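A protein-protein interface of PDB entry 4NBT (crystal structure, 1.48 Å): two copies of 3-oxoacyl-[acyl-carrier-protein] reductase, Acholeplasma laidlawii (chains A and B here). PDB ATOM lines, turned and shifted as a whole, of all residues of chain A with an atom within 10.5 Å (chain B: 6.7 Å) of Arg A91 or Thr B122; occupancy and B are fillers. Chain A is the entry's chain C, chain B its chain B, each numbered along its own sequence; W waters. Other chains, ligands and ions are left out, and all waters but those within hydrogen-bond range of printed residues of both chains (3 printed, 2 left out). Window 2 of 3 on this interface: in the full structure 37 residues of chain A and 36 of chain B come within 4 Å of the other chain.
NH2 of Arg A91 sits at hydrogen-bond distance from OG1 of Thr B122 (2.9 Å). OE2 of Glu B163 sits at hydrogen-bond distance from N of Gly A142 (2.7 Å). The side-chain carboxylate (OE1) of Glu B163 lies within hydrogen-bond range of the backbone NH (N) of Thr A90, at 2.9 Å. The guanidinium group of Arg A91 lies within hydrogen-bond range of the backbone carbonyl oxygen of Pro B118.
N of Ala A88 sits at hydrogen-bond distance from O of Gly A142 (2.9 Å). The side-chain hydroxyl (OG1) of Thr B122 lies within hydrogen-bond range of the backbone carbonyl oxygen (O) of Pro B118 (3.2 Å). The side-chain amide nitrogen (NE2) of Gln A143 sits at hydrogen-bond distance from the side-chain carboxylate (OD1) of Asp A87, 2.8 Å away.
CE of Met A89 touches CG of Glu B163, 3.6 Å away. Thr A90 touches Arg B114. SD of Met A93 touches CE1 of Phe B110, at 3.7 Å. Trp A98 touches Phe B110. OE2 of Glu B163 touches C of Ile A141, at 3.7 Å. Gln A143 touches Glu B163.
Of the printed residues of chain B, Thr A90 touches Arg B114 and Glu B163. Of the printed residues of chain B, Arg A91 touches Pro B118 and Thr B122. Lys A92 touches none of the printed residues of chain B. Glu A95 touches none of the printed residues of chain B. Printed residues of chain B within 4 Å of Trp A98: Phe B110 (3.6 Å). Gln B121 touches none of the printed residues of chain A. Of chain A, only Arg A91 (2.9 Å) comes within 4 Å of Thr B122. No residue of chain A comes within 4 Å of Asn B123. The nearest residue of chain B that does not touch Arg A91 is Arg B114 (4.3 Å). The nearest residue of chain A that does not touch Thr B122 is Met A89 (10.3 Å). The nearest printed residue of chain A that does not touch Arg B114 is Arg A91 (4.3 Å).
Of the 16 printed residues of chain B, 5 touch a printed residue of chain A. Among the printed residues, 10 pairs touch across the chains.
No position is printed for both chains.
Water W2 lies within hydrogen-bond range of the side-chain carboxylate (OE2) of Glu B163, the side-chain hydroxyl (OG1) of Thr A90, the backbone carbonyl oxygen (O) of Ala A88, the backbone NH (N) of Ala A144 and the backbone NH (N) of Gln A143. Water W3 lies within hydrogen-bond range of the guanidinium group (NH2) of Arg A91, the side-chain amide oxygen (OE1) of Gln B121 and the backbone carbonyl oxygen (O) of Pro B118. Water W1 lies within hydrogen-bond range of N of Arg A91 (2.9 Å), OE1 of Glu B163 (2.9 Å) and N of Thr A90 (3.2 Å).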
ATOM      1  N   ASP A  87      30.620 -24.963 -19.823  1.00  0.00           N
ATOM      2  CA  ASP A  87      29.913 -24.087 -20.750  1.00  0.00           C
ATOM      3  C   ASP A  87      28.429 -24.430 -20.830  1.00  0.00           C
ATOM      4  O   ASP A  87      28.028 -25.592 -20.781  1.00  0.00           O
ATOM      5  CB  ASP A  87      30.494 -24.184 -22.160  1.00  0.00           C
ATOM      6  CG  ASP A  87      31.912 -23.677 -22.268  1.00  0.00           C
ATOM      7  OD1 ASP A  87      32.413 -22.989 -21.358  1.00  0.00           O
ATOM      8  OD2 ASP A  87      32.519 -23.976 -23.322  1.00  0.00           O
ATOM      9  N   ALA A  88      27.631 -23.380 -20.996  1.00  0.00           N
ATOM     10  CA  ALA A  88      26.195 -23.502 -21.227  1.00  0.00           C
ATOM     11  C   ALA A  88      25.643 -22.149 -21.609  1.00  0.00           C
ATOM     12  O   ALA A  88      26.101 -21.143 -21.108  1.00  0.00           O
ATOM     13  CB  ALA A  88      25.497 -23.954 -19.978  1.00  0.00           C
ATOM     14  N   MET A  89      24.636 -22.135 -22.468  1.00  0.00           N
ATOM     15  CA  MET A  89      23.845 -20.929 -22.636  1.00  0.00           C
ATOM     16  C   MET A  89      23.304 -20.560 -21.273  1.00  0.00           C
ATOM     17  O   MET A  89      22.917 -21.437 -20.487  1.00  0.00           O
ATOM     18  CB  MET A  89      22.698 -21.191 -23.608  1.00  0.00           C
ATOM     19  CG  MET A  89      23.146 -21.498 -25.034  1.00  0.00           C
ATOM     20  SD  MET A  89      24.026 -20.127 -25.786  1.00  0.00           S
ATOM     21  CE  MET A  89      22.656 -19.030 -26.104  1.00  0.00           C
ATOM     22  N   THR A  90      23.258 -19.264 -20.990  1.00  0.00           N
ATOM     23  CA  THR A  90      22.790 -18.800 -19.684  1.00  0.00           C
ATOM     24  C   THR A  90      21.376 -19.301 -19.345  1.00  0.00           C
ATOM     25  O   THR A  90      21.095 -19.605 -18.194  1.00  0.00           O
ATOM     26  CB  THR A  90      22.904 -17.272 -19.610  1.00  0.00           C
ATOM     27  OG1 THR A  90      24.279 -16.925 -19.389  1.00  0.00           O
ATOM     28  CG2 THR A  90      22.093 -16.709 -18.445  1.00  0.00           C
ATOM     29  N   ARG A  91      20.532 -19.452 -20.364  1.00  0.00           N
ATOM     30  CA  ARG A  91      19.176 -19.959 -20.177  1.00  0.00           C
ATOM     31  C   ARG A  91      19.148 -21.358 -19.559  1.00  0.00           C
ATOM     32  O   ARG A  91      18.185 -21.722 -18.883  1.00  0.00           O
ATOM     33  CB  ARG A  91      18.458 -19.987 -21.525  1.00  0.00           C
ATOM     34  CG  ARG A  91      17.219 -20.872 -21.563  1.00  0.00           C
ATOM     35  CD  ARG A  91      16.707 -21.062 -22.976  1.00  0.00           C
ATOM     36  NE  ARG A  91      15.947 -19.913 -23.438  1.00  0.00           N
ATOM     37  CZ  ARG A  91      14.761 -19.561 -22.954  1.00  0.00           C
ATOM     38  NH1 ARG A  91      14.188 -20.258 -21.973  1.00  0.00           N
ATOM     39  NH2 ARG A  91      14.152 -18.499 -23.443  1.00  0.00           N
ATOM     40  N   LYS A  92      20.192 -22.148 -19.809  1.00  0.00           N
ATOM     41  CA  LYS A  92      20.254 -23.521 -19.311  1.00  0.00           C
ATOM     42  C   LYS A  92      21.315 -23.761 -18.221  1.00  0.00           C
ATOM     43  O   LYS A  92      21.332 -24.824 -17.608  1.00  0.00           O
ATOM     44  CB  LYS A  92      20.525 -24.474 -20.473  1.00  0.00           C
ATOM     45  CG  LYS A  92      19.314 -24.741 -21.351  1.00  0.00           C
ATOM     46  CD  LYS A  92      19.635 -25.743 -22.445  1.00  0.00           C
ATOM     47  CE  LYS A  92      20.089 -27.105 -21.905  1.00  0.00           C
ATOM     48  NZ  LYS A  92      19.120 -27.728 -20.961  1.00  0.00           N
ATOM     49  N   MET A  93      22.205 -22.797 -17.999  1.00  0.00           N
ATOM     50  CA  MET A  93      23.325 -22.977 -17.080  1.00  0.00           C
ATOM     51  C   MET A  93      22.851 -23.295 -15.674  1.00  0.00           C
ATOM     52  O   MET A  93      22.015 -22.609 -15.122  1.00  0.00           O
ATOM     53  CB  MET A  93      24.186 -21.716 -17.061  1.00  0.00           C
ATOM     54  CG  MET A  93      25.455 -21.825 -16.204  1.00  0.00           C
ATOM     55  SD  MET A  93      26.552 -20.409 -16.428  1.00  0.00           S
ATOM     56  CE  MET A  93      27.184 -20.768 -18.069  1.00  0.00           C
ATOM     57  N   THR A  94      23.411 -24.348 -15.092  1.00  0.00           N
ATOM     58  CA  THR A  94      22.983 -24.773 -13.763  1.00  0.00           C
ATOM     59  C   THR A  94      23.753 -24.035 -12.693  1.00  0.00           C
ATOM     60  O   THR A  94      24.836 -23.465 -12.944  1.00  0.00           O
ATOM     61  CB  THR A  94      23.203 -26.269 -13.550  1.00  0.00           C
ATOM     62  OG1 THR A  94      24.610 -26.544 -13.554  1.00  0.00           O
ATOM     63  CG2 THR A  94      22.534 -27.078 -14.636  1.00  0.00           C
ATOM     64  N   GLU A  95      23.229 -24.044 -11.478  1.00  0.00           N
ATOM     65  CA  GLU A  95      23.936 -23.435 -10.369  1.00  0.00           C
ATOM     66  C   GLU A  95      25.320 -24.074 -10.189  1.00  0.00           C
ATOM     67  O   GLU A  95      26.314 -23.378  -9.915  1.00  0.00           O
ATOM     68  CB  GLU A  95      23.107 -23.542  -9.087  1.00  0.00           C
ATOM     69  CG  GLU A  95      23.648 -22.677  -7.974  1.00  0.00           C
ATOM     70  CD  GLU A  95      22.784 -22.682  -6.724  1.00  0.00           C
ATOM     71  OE1 GLU A  95      21.714 -23.329  -6.719  1.00  0.00           O
ATOM     72  OE2 GLU A  95      23.185 -22.041  -5.735  1.00  0.00           O
ATOM     73  N   GLN A  97      27.248 -25.481 -12.499  1.00  0.00           N
ATOM     74  CA  GLN A  97      28.145 -25.010 -13.553  1.00  0.00           C
ATOM     75  C   GLN A  97      28.681 -23.619 -13.251  1.00  0.00           C
ATOM     76  O   GLN A  97      29.855 -23.322 -13.499  1.00  0.00           O
ATOM     77  CB  GLN A  97      27.440 -24.988 -14.914  1.00  0.00           C
ATOM     78  CG  GLN A  97      27.226 -26.376 -15.471  1.00  0.00           C
ATOM     79  CD  GLN A  97      26.403 -26.417 -16.736  1.00  0.00           C
ATOM     80  OE1 GLN A  97      25.374 -25.742 -16.855  1.00  0.00           O
ATOM     81  NE2 GLN A  97      26.854 -27.204 -17.701  1.00  0.00           N
ATOM     82  N   TRP A  98      27.817 -22.759 -12.746  1.00  0.00           N
ATOM     83  CA  TRP A  98      28.235 -21.436 -12.343  1.00  0.00           C
ATOM     84  C   TRP A  98      29.222 -21.558 -11.189  1.00  0.00           C
ATOM     85  O   TRP A  98      30.335 -21.045 -11.253  1.00  0.00           O
ATOM     86  CB  TRP A  98      27.038 -20.564 -11.932  1.00  0.00           C
ATOM     87  CG  TRP A  98      27.505 -19.265 -11.316  1.00  0.00           C
ATOM     88  CD1 TRP A  98      27.848 -19.060 -10.018  1.00  0.00           C
ATOM     89  CD2 TRP A  98      27.758 -18.018 -11.997  1.00  0.00           C
ATOM     90  NE1 TRP A  98      28.284 -17.767  -9.834  1.00  0.00           N
ATOM     91  CE2 TRP A  98      28.253 -17.114 -11.040  1.00  0.00           C
ATOM     92  CE3 TRP A  98      27.638 -17.597 -13.323  1.00  0.00           C
ATOM     93  CZ2 TRP A  98      28.592 -15.801 -11.352  1.00  0.00           C
ATOM     94  CZ3 TRP A  98      27.980 -16.290 -13.631  1.00  0.00           C
ATOM     95  CH2 TRP A  98      28.461 -15.413 -12.653  1.00  0.00           C
ATOM     96  N   ILE A 141      29.719 -16.340 -26.219  1.00  0.00           N
ATOM     97  CA  ILE A 141      28.476 -17.091 -26.132  1.00  0.00           C
ATOM     98  C   ILE A 141      28.694 -18.440 -25.435  1.00  0.00           C
ATOM     99  O   ILE A 141      29.658 -19.171 -25.705  1.00  0.00           O
ATOM    100  CB  ILE A 141      27.895 -17.287 -27.550  1.00  0.00           C
ATOM    101  CG1 ILE A 141      27.469 -15.929 -28.118  1.00  0.00           C
ATOM    102  CG2 ILE A 141      26.706 -18.252 -27.551  1.00  0.00           C
ATOM    103  CD1 ILE A 141      27.221 -15.942 -29.598  1.00  0.00           C
ATOM    104  N   GLY A 142      27.787 -18.754 -24.520  1.00  0.00           N
ATOM    105  CA  GLY A 142      27.837 -20.020 -23.813  1.00  0.00           C
ATOM    106  C   GLY A 142      28.789 -20.039 -22.636  1.00  0.00           C
ATOM    107  O   GLY A 142      28.992 -21.091 -22.033  1.00  0.00           O
ATOM    108  N   GLN A 143      29.365 -18.887 -22.290  1.00  0.00           N
ATOM    109  CA  GLN A 143      30.435 -18.828 -21.303  1.00  0.00           C
ATOM    110  C   GLN A 143      30.275 -17.691 -20.295  1.00  0.00           C
ATOM    111  O   GLN A 143      31.249 -17.119 -19.854  1.00  0.00           O
ATOM    112  CB  GLN A 143      31.773 -18.717 -22.021  1.00  0.00           C
ATOM    113  CG  GLN A 143      32.075 -19.945 -22.859  1.00  0.00           C
ATOM    114  CD  GLN A 143      33.550 -20.084 -23.141  1.00  0.00           C
ATOM    115  OE1 GLN A 143      34.135 -19.253 -23.843  1.00  0.00           O
ATOM    116  NE2 GLN A 143      34.168 -21.123 -22.589  1.00  0.00           N
ATOM    117  N   ALA A 144      29.057 -17.417 -19.839  1.00  0.00           N
ATOM    118  CA  ALA A 144      28.871 -16.313 -18.892  1.00  0.00           C
ATOM    119  C   ALA A 144      29.686 -16.524 -17.621  1.00  0.00           C
ATOM    120  O   ALA A 144      30.324 -15.592 -17.119  1.00  0.00           O
ATOM    121  CB  ALA A 144      27.412 -16.112 -18.559  1.00  0.00           C
ATOM    122  N   ASN A 145      29.671 -17.751 -17.096  1.00  0.00           N
ATOM    123  CA  ASN A 145      30.458 -18.059 -15.912  1.00  0.00           C
ATOM    124  C   ASN A 145      31.955 -17.822 -16.137  1.00  0.00           C
ATOM    125  O   ASN A 145      32.609 -17.124 -15.360  1.00  0.00           O
ATOM    126  CB  ASN A 145      30.135 -19.486 -15.397  1.00  0.00           C
ATOM    127  CG  ASN A 145      30.246 -20.591 -16.472  1.00  0.00           C
ATOM    128  OD1 ASN A 145      30.438 -20.336 -17.670  1.00  0.00           O
ATOM    129  ND2 ASN A 145      30.093 -21.846 -16.033  1.00  0.00           N
ATOM    130  N   PHE B 110      23.813 -12.930 -12.114  1.00  0.00           N
ATOM    131  CA  PHE B 110      23.448 -14.162 -12.810  1.00  0.00           C
ATOM    132  C   PHE B 110      22.082 -14.713 -12.402  1.00  0.00           C
ATOM    133  O   PHE B 110      21.290 -15.109 -13.257  1.00  0.00           O
ATOM    134  CB  PHE B 110      24.554 -15.230 -12.587  1.00  0.00           C
ATOM    135  CG  PHE B 110      24.195 -16.619 -13.077  1.00  0.00           C
ATOM    136  CD1 PHE B 110      24.272 -16.950 -14.427  1.00  0.00           C
ATOM    137  CD2 PHE B 110      23.829 -17.594 -12.171  1.00  0.00           C
ATOM    138  CE1 PHE B 110      23.955 -18.244 -14.860  1.00  0.00           C
ATOM    139  CE2 PHE B 110      23.520 -18.877 -12.596  1.00  0.00           C
ATOM    140  CZ  PHE B 110      23.586 -19.197 -13.934  1.00  0.00           C
ATOM    141  N   ARG B 114      19.547 -14.798 -15.576  1.00  0.00           N
ATOM    142  CA  ARG B 114      19.339 -16.062 -16.273  1.00  0.00           C
ATOM    143  C   ARG B 114      17.862 -16.358 -16.510  1.00  0.00           C
ATOM    144  O   ARG B 114      17.529 -17.207 -17.328  1.00  0.00           O
ATOM    145  CB  ARG B 114      19.981 -17.231 -15.551  1.00  0.00           C
ATOM    146  CG  ARG B 114      19.322 -17.565 -14.249  1.00  0.00           C
ATOM    147  CD  ARG B 114      19.887 -18.826 -13.625  1.00  0.00           C
ATOM    148  NE  ARG B 114      18.965 -19.247 -12.583  1.00  0.00           N
ATOM    149  CZ  ARG B 114      17.914 -20.034 -12.796  1.00  0.00           C
ATOM    150  NH1 ARG B 114      17.690 -20.546 -14.006  1.00  0.00           N
ATOM    151  NH2 ARG B 114      17.111 -20.327 -11.790  1.00  0.00           N
ATOM    152  N   LEU B 115      16.982 -15.672 -15.781  1.00  0.00           N
ATOM    153  CA  LEU B 115      15.532 -15.735 -16.036  1.00  0.00           C
ATOM    154  C   LEU B 115      15.081 -14.596 -16.953  1.00  0.00           C
ATOM    155  O   LEU B 115      14.378 -14.810 -17.957  1.00  0.00           O
ATOM    156  CB  LEU B 115      14.758 -15.654 -14.714  1.00  0.00           C
ATOM    157  CG  LEU B 115      15.142 -16.751 -13.720  1.00  0.00           C
ATOM    158  CD1 LEU B 115      14.510 -16.533 -12.350  1.00  0.00           C
ATOM    159  CD2 LEU B 115      14.753 -18.117 -14.252  1.00  0.00           C
ATOM    160  N   GLY B 117      16.822 -12.382 -18.957  1.00  0.00           N
ATOM    161  CA  GLY B 117      17.469 -12.207 -20.243  1.00  0.00           C
ATOM    162  C   GLY B 117      16.919 -13.117 -21.326  1.00  0.00           C
ATOM    163  O   GLY B 117      16.603 -12.658 -22.428  1.00  0.00           O
ATOM    164  N   PRO B 118      16.818 -14.419 -21.035  1.00  0.00           N
ATOM    165  CA  PRO B 118      16.244 -15.306 -22.046  1.00  0.00           C
ATOM    166  C   PRO B 118      14.792 -14.934 -22.367  1.00  0.00           C
ATOM    167  O   PRO B 118      14.370 -15.054 -23.514  1.00  0.00           O
ATOM    168  CB  PRO B 118      16.380 -16.691 -21.400  1.00  0.00           C
ATOM    169  CG  PRO B 118      17.640 -16.554 -20.527  1.00  0.00           C
ATOM    170  CD  PRO B 118      17.470 -15.167 -19.943  1.00  0.00           C
ATOM    171  N   GLN B 119      14.057 -14.448 -21.369  1.00  0.00           N
ATOM    172  CA  GLN B 119      12.702 -13.952 -21.601  1.00  0.00           C
ATOM    173  C   GLN B 119      12.677 -12.752 -22.551  1.00  0.00           C
ATOM    174  O   GLN B 119      11.797 -12.635 -23.395  1.00  0.00           O
ATOM    175  CB  GLN B 119      12.033 -13.632 -20.257  1.00  0.00           C
ATOM    176  CG  GLN B 119      10.660 -12.952 -20.313  1.00  0.00           C
ATOM    177  CD  GLN B 119      10.648 -11.437 -20.162  1.00  0.00           C
ATOM    178  OE1 GLN B 119       9.583 -10.833 -20.252  1.00  0.00           O
ATOM    179  NE2 GLN B 119      11.803 -10.816 -19.923  1.00  0.00           N
ATOM    180  N   MET B 120      13.665 -11.870 -22.446  1.00  0.00           N
ATOM    181  CA  MET B 120      13.794 -10.773 -23.393  1.00  0.00           C
ATOM    182  C   MET B 120      14.102 -11.324 -24.777  1.00  0.00           C
ATOM    183  O   MET B 120      13.540 -10.873 -25.767  1.00  0.00           O
ATOM    184  CB  MET B 120      14.897  -9.803 -22.984  1.00  0.00           C
ATOM    185  CG  MET B 120      14.594  -8.995 -21.767  1.00  0.00           C
ATOM    186  SD  MET B 120      16.046  -8.131 -21.160  1.00  0.00           S
ATOM    187  CE  MET B 120      15.340  -7.049 -19.931  1.00  0.00           C
ATOM    188  N   GLN B 121      14.989 -12.313 -24.848  1.00  0.00           N
ATOM    189  CA  GLN B 121      15.356 -12.880 -26.146  1.00  0.00           C
ATOM    190  C   GLN B 121      14.143 -13.500 -26.829  1.00  0.00           C
ATOM    191  O   GLN B 121      13.936 -13.316 -28.018  1.00  0.00           O
ATOM    192  CB  GLN B 121      16.466 -13.919 -25.994  1.00  0.00           C
ATOM    193  CG  GLN B 121      17.142 -14.369 -27.307  1.00  0.00           C
ATOM    194  CD  GLN B 121      16.420 -15.472 -28.025  1.00  0.00           C
ATOM    195  OE1 GLN B 121      15.708 -16.272 -27.416  1.00  0.00           O
ATOM    196  NE2 GLN B 121      16.621 -15.544 -29.343  1.00  0.00           N
ATOM    197  N   THR B 122      13.329 -14.208 -26.049  1.00  0.00           N
ATOM    198  CA  THR B 122      12.143 -14.877 -26.561  1.00  0.00           C
ATOM    199  C   THR B 122      11.074 -13.855 -26.975  1.00  0.00           C
ATOM    200  O   THR B 122      10.407 -14.014 -28.011  1.00  0.00           O
ATOM    201  CB  THR B 122      11.630 -15.884 -25.491  1.00  0.00           C
ATOM    202  OG1 THR B 122      12.588 -16.946 -25.367  1.00  0.00           O
ATOM    203  CG2 THR B 122      10.308 -16.479 -25.873  1.00  0.00           C
ATOM    204  N   ASN B 123      10.933 -12.788 -26.202  1.00  0.00           N
ATOM    205  CA  ASN B 123      10.024 -11.694 -26.582  1.00  0.00           C
ATOM    206  C   ASN B 123      10.506 -10.909 -27.786  1.00  0.00           C
ATOM    207  O   ASN B 123       9.715 -10.215 -28.439  1.00  0.00           O
ATOM    208  CB  ASN B 123       9.888 -10.684 -25.454  1.00  0.00           C
ATOM    209  CG  ASN B 123       9.106 -11.210 -24.291  1.00  0.00           C
ATOM    210  OD1 ASN B 123       8.354 -12.172 -24.420  1.00  0.00           O
ATOM    211  ND2 ASN B 123       9.265 -10.565 -23.137  1.00  0.00           N
ATOM    212  N   GLY B 124      11.816 -10.957 -28.024  1.00  0.00           N
ATOM    213  CA  GLY B 124      12.431 -10.262 -29.132  1.00  0.00           C
ATOM    214  C   GLY B 124      12.903  -8.848 -28.850  1.00  0.00           C
ATOM    215  O   GLY B 124      13.264  -8.117 -29.779  1.00  0.00           O
ATOM    216  N   TYR B 125      12.899  -8.455 -27.579  1.00  0.00           N
ATOM    217  CA  TYR B 125      13.255  -7.093 -27.198  1.00  0.00           C
ATOM    218  C   TYR B 125      13.663  -7.012 -25.739  1.00  0.00           C
ATOM    219  O   TYR B 125      13.077  -7.664 -24.888  1.00  0.00           O
ATOM    220  CB  TYR B 125      12.060  -6.140 -27.439  1.00  0.00           C
ATOM    221  CG  TYR B 125      12.327  -4.705 -27.030  1.00  0.00           C
ATOM    222  CD1 TYR B 125      12.890  -3.805 -27.923  1.00  0.00           C
ATOM    223  CD2 TYR B 125      12.018  -4.252 -25.753  1.00  0.00           C
ATOM    224  CE1 TYR B 125      13.146  -2.490 -27.562  1.00  0.00           C
ATOM    225  CE2 TYR B 125      12.273  -2.941 -25.378  1.00  0.00           C
ATOM    226  CZ  TYR B 125      12.840  -2.065 -26.287  1.00  0.00           C
ATOM    227  OH  TYR B 125      13.091  -0.759 -25.927  1.00  0.00           O
ATOM    228  N   GLU B 163      24.819 -13.178 -26.495  1.00  0.00           N
ATOM    229  CA  GLU B 163      23.910 -14.325 -26.362  1.00  0.00           C
ATOM    230  C   GLU B 163      22.443 -13.952 -26.553  1.00  0.00           C
ATOM    231  O   GLU B 163      21.703 -14.654 -27.258  1.00  0.00           O
ATOM    232  CB  GLU B 163      24.051 -14.976 -24.987  1.00  0.00           C
ATOM    233  CG  GLU B 163      24.715 -16.287 -25.006  1.00  0.00           C
ATOM    234  CD  GLU B 163      24.763 -16.955 -23.642  1.00  0.00           C
ATOM    235  OE1 GLU B 163      23.693 -17.139 -22.968  1.00  0.00           O
ATOM    236  OE2 GLU B 163      25.890 -17.284 -23.277  1.00  0.00           O
ATOM    237  N   PHE B 164      22.007 -12.854 -25.941  1.00  0.00           N
ATOM    238  CA  PHE B 164      20.580 -12.550 -25.900  1.00  0.00           C
ATOM    239  C   PHE B 164      20.108 -11.880 -27.175  1.00  0.00           C
ATOM    240  O   PHE B 164      18.898 -11.720 -27.356  1.00  0.00           O
ATOM    241  CB  PHE B 164      20.225 -11.687 -24.684  1.00  0.00           C
ATOM    242  CG  PHE B 164      20.481 -12.358 -23.343  1.00  0.00           C
ATOM    243  CD1 PHE B 164      20.386 -13.734 -23.178  1.00  0.00           C
ATOM    244  CD2 PHE B 164      20.840 -11.605 -22.249  1.00  0.00           C
ATOM    245  CE1 PHE B 164      20.619 -14.327 -21.923  1.00  0.00           C
ATOM    246  CE2 PHE B 164      21.080 -12.185 -21.005  1.00  0.00           C
ATOM    247  CZ  PHE B 164      20.974 -13.548 -20.851  1.00  0.00           C
ATOM    248  N   ALA B 169      17.058 -11.239 -32.139  1.00  0.00           N
ATOM    249  CA  ALA B 169      16.386 -10.581 -31.023  1.00  0.00           C
ATOM    250  C   ALA B 169      17.015  -9.231 -30.730  1.00  0.00           C
ATOM    251  O   ALA B 169      18.231  -9.117 -30.632  1.00  0.00           O
ATOM    252  CB  ALA B 169      16.423 -11.468 -29.789  1.00  0.00           C
ATOM    253  N   VAL B 171      17.784  -7.346 -28.252  1.00  0.00           N
ATOM    254  CA  VAL B 171      18.124  -7.239 -26.835  1.00  0.00           C
ATOM    255  C   VAL B 171      19.515  -6.648 -26.744  1.00  0.00           C
ATOM    256  O   VAL B 171      20.445  -7.137 -27.385  1.00  0.00           O
ATOM    257  CB  VAL B 171      18.129  -8.607 -26.137  1.00  0.00           C
ATOM    258  CG1 VAL B 171      18.457  -8.454 -24.640  1.00  0.00           C
ATOM    259  CG2 VAL B 171      16.784  -9.302 -26.315  1.00  0.00           C
HETATM  260  O   HOH W   1      20.903 -17.936 -22.783  1.00  0.00           O
HETATM  261  O   HOH W   2      26.300 -18.282 -20.853  1.00  0.00           O
HETATM  262  O   HOH W   3      16.208 -17.579 -25.019  1.00  0.00           O
